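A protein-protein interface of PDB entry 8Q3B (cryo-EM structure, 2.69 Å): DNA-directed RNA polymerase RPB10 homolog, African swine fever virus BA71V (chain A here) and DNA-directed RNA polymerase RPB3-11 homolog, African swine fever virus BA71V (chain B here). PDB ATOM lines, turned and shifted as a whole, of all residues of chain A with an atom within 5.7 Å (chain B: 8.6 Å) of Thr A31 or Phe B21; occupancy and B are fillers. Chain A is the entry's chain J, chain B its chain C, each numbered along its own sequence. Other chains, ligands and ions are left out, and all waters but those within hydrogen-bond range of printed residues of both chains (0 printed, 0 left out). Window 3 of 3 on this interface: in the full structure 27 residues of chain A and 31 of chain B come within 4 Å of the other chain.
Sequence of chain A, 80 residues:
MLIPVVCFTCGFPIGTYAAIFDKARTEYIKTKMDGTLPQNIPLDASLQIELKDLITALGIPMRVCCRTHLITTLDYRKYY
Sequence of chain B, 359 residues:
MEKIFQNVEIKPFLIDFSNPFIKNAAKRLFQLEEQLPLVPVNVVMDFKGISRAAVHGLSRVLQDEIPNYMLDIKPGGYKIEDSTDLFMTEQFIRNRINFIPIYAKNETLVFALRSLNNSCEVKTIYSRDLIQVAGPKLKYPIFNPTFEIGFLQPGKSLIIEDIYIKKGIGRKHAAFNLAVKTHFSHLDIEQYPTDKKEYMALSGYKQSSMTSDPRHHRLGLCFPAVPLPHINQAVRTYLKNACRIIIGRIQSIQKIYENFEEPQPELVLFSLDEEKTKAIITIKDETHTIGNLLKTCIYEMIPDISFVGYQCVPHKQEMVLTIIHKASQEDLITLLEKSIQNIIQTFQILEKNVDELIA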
ATOM      1  N   ALA A  24     -23.980 -32.705 -23.206  1.00  0.00           N
ATOM      2  CA  ALA A  24     -24.046 -31.565 -22.298  1.00  0.00           C
ATOM      3  C   ALA A  24     -25.140 -31.766 -21.262  1.00  0.00           C
ATOM      4  O   ALA A  24     -24.889 -31.691 -20.053  1.00  0.00           O
ATOM      5  CB  ALA A  24     -24.283 -30.281 -23.092  1.00  0.00           C
ATOM      6  N   THR A  26     -26.447 -34.359 -19.955  1.00  0.00           N
ATOM      7  CA  THR A  26     -25.996 -35.258 -18.900  1.00  0.00           C
ATOM      8  C   THR A  26     -25.209 -34.488 -17.852  1.00  0.00           C
ATOM      9  O   THR A  26     -25.639 -34.360 -16.699  1.00  0.00           O
ATOM     10  CB  THR A  26     -25.148 -36.386 -19.497  1.00  0.00           C
ATOM     11  OG1 THR A  26     -25.949 -37.172 -20.388  1.00  0.00           O
ATOM     12  CG2 THR A  26     -24.595 -37.283 -18.399  1.00  0.00           C
ATOM     13  N   GLU A  27     -24.082 -33.901 -18.260  1.00  0.00           N
ATOM     14  CA  GLU A  27     -23.263 -33.158 -17.313  1.00  0.00           C
ATOM     15  C   GLU A  27     -24.113 -32.141 -16.570  1.00  0.00           C
ATOM     16  O   GLU A  27     -24.154 -32.129 -15.333  1.00  0.00           O
ATOM     17  CB  GLU A  27     -22.110 -32.466 -18.042  1.00  0.00           C
ATOM     18  CG  GLU A  27     -20.796 -33.223 -17.986  1.00  0.00           C
ATOM     19  CD  GLU A  27     -20.932 -34.660 -18.448  1.00  0.00           C
ATOM     20  OE1 GLU A  27     -21.848 -34.944 -19.246  1.00  0.00           O
ATOM     21  OE2 GLU A  27     -20.121 -35.504 -18.013  1.00  0.00           O
ATOM     22  N   TYR A  28     -24.861 -31.329 -17.318  1.00  0.00           N
ATOM     23  CA  TYR A  28     -25.681 -30.303 -16.690  1.00  0.00           C
ATOM     24  C   TYR A  28     -26.547 -30.913 -15.602  1.00  0.00           C
ATOM     25  O   TYR A  28     -26.527 -30.464 -14.448  1.00  0.00           O
ATOM     26  CB  TYR A  28     -26.546 -29.608 -17.742  1.00  0.00           C
ATOM     27  CG  TYR A  28     -27.375 -28.470 -17.196  1.00  0.00           C
ATOM     28  CD1 TYR A  28     -26.773 -27.357 -16.628  1.00  0.00           C
ATOM     29  CD2 TYR A  28     -28.760 -28.510 -17.246  1.00  0.00           C
ATOM     30  CE1 TYR A  28     -27.526 -26.315 -16.129  1.00  0.00           C
ATOM     31  CE2 TYR A  28     -29.522 -27.474 -16.750  1.00  0.00           C
ATOM     32  CZ  TYR A  28     -28.901 -26.379 -16.192  1.00  0.00           C
ATOM     33  OH  TYR A  28     -29.658 -25.344 -15.695  1.00  0.00           O
ATOM     34  N   ILE A  29     -27.259 -31.991 -15.934  1.00  0.00           N
ATOM     35  CA  ILE A  29     -28.169 -32.589 -14.964  1.00  0.00           C
ATOM     36  C   ILE A  29     -27.404 -32.917 -13.691  1.00  0.00           C
ATOM     37  O   ILE A  29     -27.789 -32.507 -12.588  1.00  0.00           O
ATOM     38  CB  ILE A  29     -28.838 -33.842 -15.560  1.00  0.00           C
ATOM     39  CG1 ILE A  29     -29.892 -33.470 -16.613  1.00  0.00           C
ATOM     40  CG2 ILE A  29     -29.481 -34.674 -14.462  1.00  0.00           C
ATOM     41  CD1 ILE A  29     -30.837 -32.352 -16.220  1.00  0.00           C
ATOM     42  N   LYS A  30     -26.262 -33.589 -13.840  1.00  0.00           N
ATOM     43  CA  LYS A  30     -25.466 -33.964 -12.679  1.00  0.00           C
ATOM     44  C   LYS A  30     -25.216 -32.748 -11.799  1.00  0.00           C
ATOM     45  O   LYS A  30     -25.496 -32.760 -10.594  1.00  0.00           O
ATOM     46  CB  LYS A  30     -24.146 -34.589 -13.138  1.00  0.00           C
ATOM     47  CG  LYS A  30     -24.170 -36.107 -13.222  1.00  0.00           C
ATOM     48  CD  LYS A  30     -22.765 -36.691 -13.283  1.00  0.00           C
ATOM     49  CE  LYS A  30     -22.189 -36.613 -14.689  1.00  0.00           C
ATOM     50  NZ  LYS A  30     -22.337 -37.892 -15.437  1.00  0.00           N
ATOM     51  N   THR A  31     -24.742 -31.661 -12.410  1.00  0.00           N
ATOM     52  CA  THR A  31     -24.392 -30.476 -11.639  1.00  0.00           C
ATOM     53  C   THR A  31     -25.583 -29.984 -10.832  1.00  0.00           C
ATOM     54  O   THR A  31     -25.448 -29.626  -9.656  1.00  0.00           O
ATOM     55  CB  THR A  31     -23.878 -29.377 -12.571  1.00  0.00           C
ATOM     56  OG1 THR A  31     -22.752 -29.865 -13.310  1.00  0.00           O
ATOM     57  CG2 THR A  31     -23.459 -28.152 -11.772  1.00  0.00           C
ATOM     58  N   LYS A  32     -26.766 -29.958 -11.448  1.00  0.00           N
ATOM     59  CA  LYS A  32     -27.934 -29.455 -10.736  1.00  0.00           C
ATOM     60  C   LYS A  32     -28.328 -30.404  -9.615  1.00  0.00           C
ATOM     61  O   LYS A  32     -28.806 -29.973  -8.559  1.00  0.00           O
ATOM     62  CB  LYS A  32     -29.095 -29.245 -11.707  1.00  0.00           C
ATOM     63  CG  LYS A  32     -28.731 -28.405 -12.923  1.00  0.00           C
ATOM     64  CD  LYS A  32     -28.180 -27.039 -12.539  1.00  0.00           C
ATOM     65  CE  LYS A  32     -29.201 -26.195 -11.802  1.00  0.00           C
ATOM     66  NZ  LYS A  32     -28.666 -24.844 -11.488  1.00  0.00           N
ATOM     67  N   MET A  33     -28.135 -31.703  -9.831  1.00  0.00           N
ATOM     68  CA  MET A  33     -28.456 -32.719  -8.833  1.00  0.00           C
ATOM     69  C   MET A  33     -27.195 -33.040  -8.028  1.00  0.00           C
ATOM     70  O   MET A  33     -26.660 -34.150  -8.041  1.00  0.00           O
ATOM     71  CB  MET A  33     -29.034 -33.948  -9.518  1.00  0.00           C
ATOM     72  CG  MET A  33     -30.555 -33.914  -9.648  1.00  0.00           C
ATOM     73  SD  MET A  33     -31.276 -35.311 -10.536  1.00  0.00           S
ATOM     74  CE  MET A  33     -29.843 -36.337 -10.842  1.00  0.00           C
ATOM     75  N   ASP A  34     -26.726 -32.021  -7.313  1.00  0.00           N
ATOM     76  CA  ASP A  34     -25.476 -32.127  -6.574  1.00  0.00           C
ATOM     77  C   ASP A  34     -25.594 -33.166  -5.464  1.00  0.00           C
ATOM     78  O   ASP A  34     -26.644 -33.323  -4.834  1.00  0.00           O
ATOM     79  CB  ASP A  34     -25.096 -30.768  -5.981  1.00  0.00           C
ATOM     80  CG  ASP A  34     -23.594 -30.534  -5.961  1.00  0.00           C
ATOM     81  OD1 ASP A  34     -22.839 -31.397  -6.455  1.00  0.00           O
ATOM     82  OD2 ASP A  34     -23.168 -29.477  -5.449  1.00  0.00           O
ATOM     83  N   LEU A  54     -29.387 -24.133 -21.923  1.00  0.00           N
ATOM     84  CA  LEU A  54     -28.454 -25.007 -22.626  1.00  0.00           C
ATOM     85  C   LEU A  54     -28.782 -25.070 -24.114  1.00  0.00           C
ATOM     86  O   LEU A  54     -27.898 -24.917 -24.968  1.00  0.00           O
ATOM     87  CB  LEU A  54     -28.490 -26.404 -22.006  1.00  0.00           C
ATOM     88  CG  LEU A  54     -27.218 -27.239 -22.145  1.00  0.00           C
ATOM     89  CD1 LEU A  54     -26.151 -26.751 -21.182  1.00  0.00           C
ATOM     90  CD2 LEU A  54     -27.524 -28.707 -21.910  1.00  0.00           C
ATOM     91  N   ASP B  16     -22.850 -20.992 -28.898  1.00  0.00           N
ATOM     92  CA  ASP B  16     -22.311 -20.167 -27.818  1.00  0.00           C
ATOM     93  C   ASP B  16     -21.347 -21.021 -27.007  1.00  0.00           C
ATOM     94  O   ASP B  16     -21.760 -21.795 -26.140  1.00  0.00           O
ATOM     95  CB  ASP B  16     -23.433 -19.615 -26.949  1.00  0.00           C
ATOM     96  CG  ASP B  16     -22.917 -18.805 -25.777  1.00  0.00           C
ATOM     97  OD1 ASP B  16     -21.832 -18.202 -25.903  1.00  0.00           O
ATOM     98  OD2 ASP B  16     -23.596 -18.774 -24.729  1.00  0.00           O
ATOM     99  N   PHE B  17     -20.051 -20.881 -27.286  1.00  0.00           N
ATOM    100  CA  PHE B  17     -19.037 -21.653 -26.582  1.00  0.00           C
ATOM    101  C   PHE B  17     -18.756 -21.126 -25.182  1.00  0.00           C
ATOM    102  O   PHE B  17     -18.038 -21.785 -24.424  1.00  0.00           O
ATOM    103  CB  PHE B  17     -17.740 -21.674 -27.393  1.00  0.00           C
ATOM    104  CG  PHE B  17     -17.776 -22.614 -28.563  1.00  0.00           C
ATOM    105  CD1 PHE B  17     -17.925 -23.976 -28.368  1.00  0.00           C
ATOM    106  CD2 PHE B  17     -17.666 -22.135 -29.856  1.00  0.00           C
ATOM    107  CE1 PHE B  17     -17.962 -24.842 -29.440  1.00  0.00           C
ATOM    108  CE2 PHE B  17     -17.701 -22.999 -30.933  1.00  0.00           C
ATOM    109  CZ  PHE B  17     -17.849 -24.353 -30.723  1.00  0.00           C
ATOM    110  N   SER B  18     -19.297 -19.961 -24.821  1.00  0.00           N
ATOM    111  CA  SER B  18     -19.141 -19.466 -23.460  1.00  0.00           C
ATOM    112  C   SER B  18     -19.813 -20.379 -22.444  1.00  0.00           C
ATOM    113  O   SER B  18     -19.470 -20.329 -21.259  1.00  0.00           O
ATOM    114  CB  SER B  18     -19.711 -18.052 -23.346  1.00  0.00           C
ATOM    115  OG  SER B  18     -21.126 -18.077 -23.294  1.00  0.00           O
ATOM    116  N   ASN B  19     -20.758 -21.203 -22.877  1.00  0.00           N
ATOM    117  CA  ASN B  19     -21.400 -22.152 -21.980  1.00  0.00           C
ATOM    118  C   ASN B  19     -20.435 -23.293 -21.685  1.00  0.00           C
ATOM    119  O   ASN B  19     -20.019 -23.992 -22.619  1.00  0.00           O
ATOM    120  CB  ASN B  19     -22.684 -22.683 -22.611  1.00  0.00           C
ATOM    121  CG  ASN B  19     -23.579 -23.383 -21.612  1.00  0.00           C
ATOM    122  OD1 ASN B  19     -23.282 -24.487 -21.162  1.00  0.00           O
ATOM    123  ND2 ASN B  19     -24.688 -22.743 -21.264  1.00  0.00           N
ATOM    124  N   PRO B  20     -20.048 -23.523 -20.427  1.00  0.00           N
ATOM    125  CA  PRO B  20     -19.023 -24.549 -20.167  1.00  0.00           C
ATOM    126  C   PRO B  20     -19.426 -25.941 -20.620  1.00  0.00           C
ATOM    127  O   PRO B  20     -18.592 -26.678 -21.163  1.00  0.00           O
ATOM    128  CB  PRO B  20     -18.836 -24.476 -18.646  1.00  0.00           C
ATOM    129  CG  PRO B  20     -20.099 -23.883 -18.130  1.00  0.00           C
ATOM    130  CD  PRO B  20     -20.561 -22.927 -19.180  1.00  0.00           C
ATOM    131  N   PHE B  21     -20.689 -26.320 -20.423  1.00  0.00           N
ATOM    132  CA  PHE B  21     -21.111 -27.673 -20.767  1.00  0.00           C
ATOM    133  C   PHE B  21     -21.067 -27.900 -22.272  1.00  0.00           C
ATOM    134  O   PHE B  21     -20.576 -28.937 -22.734  1.00  0.00           O
ATOM    135  CB  PHE B  21     -22.514 -27.934 -20.222  1.00  0.00           C
ATOM    136  CG  PHE B  21     -22.642 -27.696 -18.746  1.00  0.00           C
ATOM    137  CD1 PHE B  21     -22.195 -28.639 -17.838  1.00  0.00           C
ATOM    138  CD2 PHE B  21     -23.206 -26.527 -18.265  1.00  0.00           C
ATOM    139  CE1 PHE B  21     -22.309 -28.422 -16.481  1.00  0.00           C
ATOM    140  CE2 PHE B  21     -23.322 -26.306 -16.909  1.00  0.00           C
ATOM    141  CZ  PHE B  21     -22.874 -27.254 -16.016  1.00  0.00           C
ATOM    142  N   ILE B  22     -21.572 -26.942 -23.051  1.00  0.00           N
ATOM    143  CA  ILE B  22     -21.543 -27.079 -24.504  1.00  0.00           C
ATOM    144  C   ILE B  22     -20.107 -27.143 -24.999  1.00  0.00           C
ATOM    145  O   ILE B  22     -19.766 -27.959 -25.863  1.00  0.00           O
ATOM    146  CB  ILE B  22     -22.317 -25.923 -25.165  1.00  0.00           C
ATOM    147  CG1 ILE B  22     -23.778 -25.916 -24.706  1.00  0.00           C
ATOM    148  CG2 ILE B  22     -22.235 -26.024 -26.682  1.00  0.00           C
ATOM    149  CD1 ILE B  22     -24.535 -27.192 -25.010  1.00  0.00           C
ATOM    150  N   LYS B  23     -19.241 -26.280 -24.462  1.00  0.00           N
ATOM    151  CA  LYS B  23     -17.844 -26.279 -24.879  1.00  0.00           C
ATOM    152  C   LYS B  23     -17.189 -27.624 -24.592  1.00  0.00           C
ATOM    153  O   LYS B  23     -16.516 -28.200 -25.457  1.00  0.00           O
ATOM    154  CB  LYS B  23     -17.096 -25.150 -24.166  1.00  0.00           C
ATOM    155  CG  LYS B  23     -15.602 -25.100 -24.441  1.00  0.00           C
ATOM    156  CD  LYS B  23     -14.918 -24.070 -23.559  1.00  0.00           C
ATOM    157  CE  LYS B  23     -13.744 -23.416 -24.269  1.00  0.00           C
ATOM    158  NZ  LYS B  23     -12.831 -24.418 -24.886  1.00  0.00           N
ATOM    159  N   ASN B  24     -17.382 -28.144 -23.378  1.00  0.00           N
ATOM    160  CA  ASN B  24     -16.766 -29.416 -23.016  1.00  0.00           C
ATOM    161  C   ASN B  24     -17.290 -30.544 -23.894  1.00  0.00           C
ATOM    162  O   ASN B  24     -16.514 -31.369 -24.394  1.00  0.00           O
ATOM    163  CB  ASN B  24     -17.025 -29.721 -21.541  1.00  0.00           C
ATOM    164  CG  ASN B  24     -16.210 -28.844 -20.614  1.00  0.00           C
ATOM    165  OD1 ASN B  24     -15.186 -28.285 -21.009  1.00  0.00           O
ATOM    166  ND2 ASN B  24     -16.661 -28.715 -19.372  1.00  0.00           N
ATOM    167  N   ALA B  25     -18.608 -30.596 -24.100  1.00  0.00           N
ATOM    168  CA  ALA B  25     -19.181 -31.663 -24.909  1.00  0.00           C
ATOM    169  C   ALA B  25     -18.673 -31.602 -26.341  1.00  0.00           C
ATOM    170  O   ALA B  25     -18.314 -32.633 -26.924  1.00  0.00           O
ATOM    171  CB  ALA B  25     -20.708 -31.580 -24.879  1.00  0.00           C
ATOM    172  N   ALA B  26     -18.634 -30.404 -26.929  1.00  0.00           N
ATOM    173  CA  ALA B  26     -18.158 -30.272 -28.300  1.00  0.00           C
ATOM    174  C   ALA B  26     -16.699 -30.686 -28.411  1.00  0.00           C
ATOM    175  O   ALA B  26     -16.327 -31.463 -29.299  1.00  0.00           O
ATOM    176  CB  ALA B  26     -18.350 -28.834 -28.782  1.00  0.00           C
ATOM    177  N   LYS B  27     -15.855 -30.196 -27.500  1.00  0.00           N
ATOM    178  CA  LYS B  27     -14.439 -30.543 -27.558  1.00  0.00           C
ATOM    179  C   LYS B  27     -14.233 -32.043 -27.408  1.00  0.00           C
ATOM    180  O   LYS B  27     -13.408 -32.636 -28.112  1.00  0.00           O
ATOM    181  CB  LYS B  27     -13.666 -29.791 -26.477  1.00  0.00           C
ATOM    182  CG  LYS B  27     -12.160 -29.931 -26.608  1.00  0.00           C
ATOM    183  CD  LYS B  27     -11.419 -28.955 -25.714  1.00  0.00           C
ATOM    184  CE  LYS B  27      -9.911 -29.128 -25.831  1.00  0.00           C
ATOM    185  NZ  LYS B  27      -9.435 -29.074 -27.241  1.00  0.00           N
ATOM    186  N   ARG B  28     -14.969 -32.677 -26.493  1.00  0.00           N
ATOM    187  CA  ARG B  28     -14.779 -34.105 -26.265  1.00  0.00           C
ATOM    188  C   ARG B  28     -15.266 -34.926 -27.454  1.00  0.00           C
ATOM    189  O   ARG B  28     -14.563 -35.827 -27.925  1.00  0.00           O
ATOM    190  CB  ARG B  28     -15.501 -34.528 -24.984  1.00  0.00           C
ATOM    191  CG  ARG B  28     -15.235 -35.982 -24.583  1.00  0.00           C
ATOM    192  CD  ARG B  28     -15.725 -36.370 -23.172  1.00  0.00           C
ATOM    193  NE  ARG B  28     -15.648 -35.355 -22.121  1.00  0.00           N
ATOM    194  CZ  ARG B  28     -14.652 -34.497 -21.927  1.00  0.00           C
ATOM    195  NH1 ARG B  28     -13.514 -34.582 -22.596  1.00  0.00           N
ATOM    196  NH2 ARG B  28     -14.792 -33.546 -21.007  1.00  0.00           N
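O of Glu A27 lies within hydrogen-bond range of OG1 of Thr A31 (3.3 Å).
OD1 of Asn B19 sits at hydrogen-bond distance from N of Phe B21, at 3.3 Å.
Ala A24 touches Phe B21.
Ile B22 touches Ala A24.
Ala B25 touches Ala A24 (CB to N, 3.8 Å).
CD1 of Phe B21 touches CB of Glu A27 (3.8 Å).
Tyr A28 touches Phe B21 (CD1 to CE2, 3.6 Å).
OG1 of Thr A31 touches CE1 of Phe B21, 3.5 Å away.
Asn B19 touches Leu A54 (OD1 to CD1, 3.7 Å).
Leu A54 touches Phe B21.
Ile B22 touches Leu A54.
Thr A31 touches just one residue of chain B: Phe B21 (3.5 Å).
Of chain A, only Ala A24 (3.96 Å), Glu A27 (3.8 Å), Tyr A28 (3.6 Å), Thr A31 (3.5 Å) and Leu A54 (3.9 Å) come within 4 Å of Phe B21.
Of the printed residues of chain B, Leu A54 touches Asn B19 (3.7 Å), Phe B21 (3.9 Å) and Ile B22 (3.9 Å).
Printed residues of chain A within 4 Å of Ile B22: Ala A24 and Leu A54.
Ile A29 touches none of the printed residues of chain B.
Lys B23 touches none of the printed residues of chain A.
The nearest printed residue of chain B that does not touch Ala A24 is Asn B19 (6.2 Å).
Of the 11 printed residues of chain A, 5 touch a printed residue of chain B.
Hydrophobic or aromatic side chains of chain A that line the printed part of chain B: Ala A24, Tyr A28 and Leu A54.
Of the 13 printed residues of chain B, 4 touch a printed residue of chain A.
Hydrophobic or aromatic side chains of chain B that line the printed part of chain A: Phe B21, Ile B22 and Ala B25.
Among the printed residues, 9 pairs touch across the chains.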
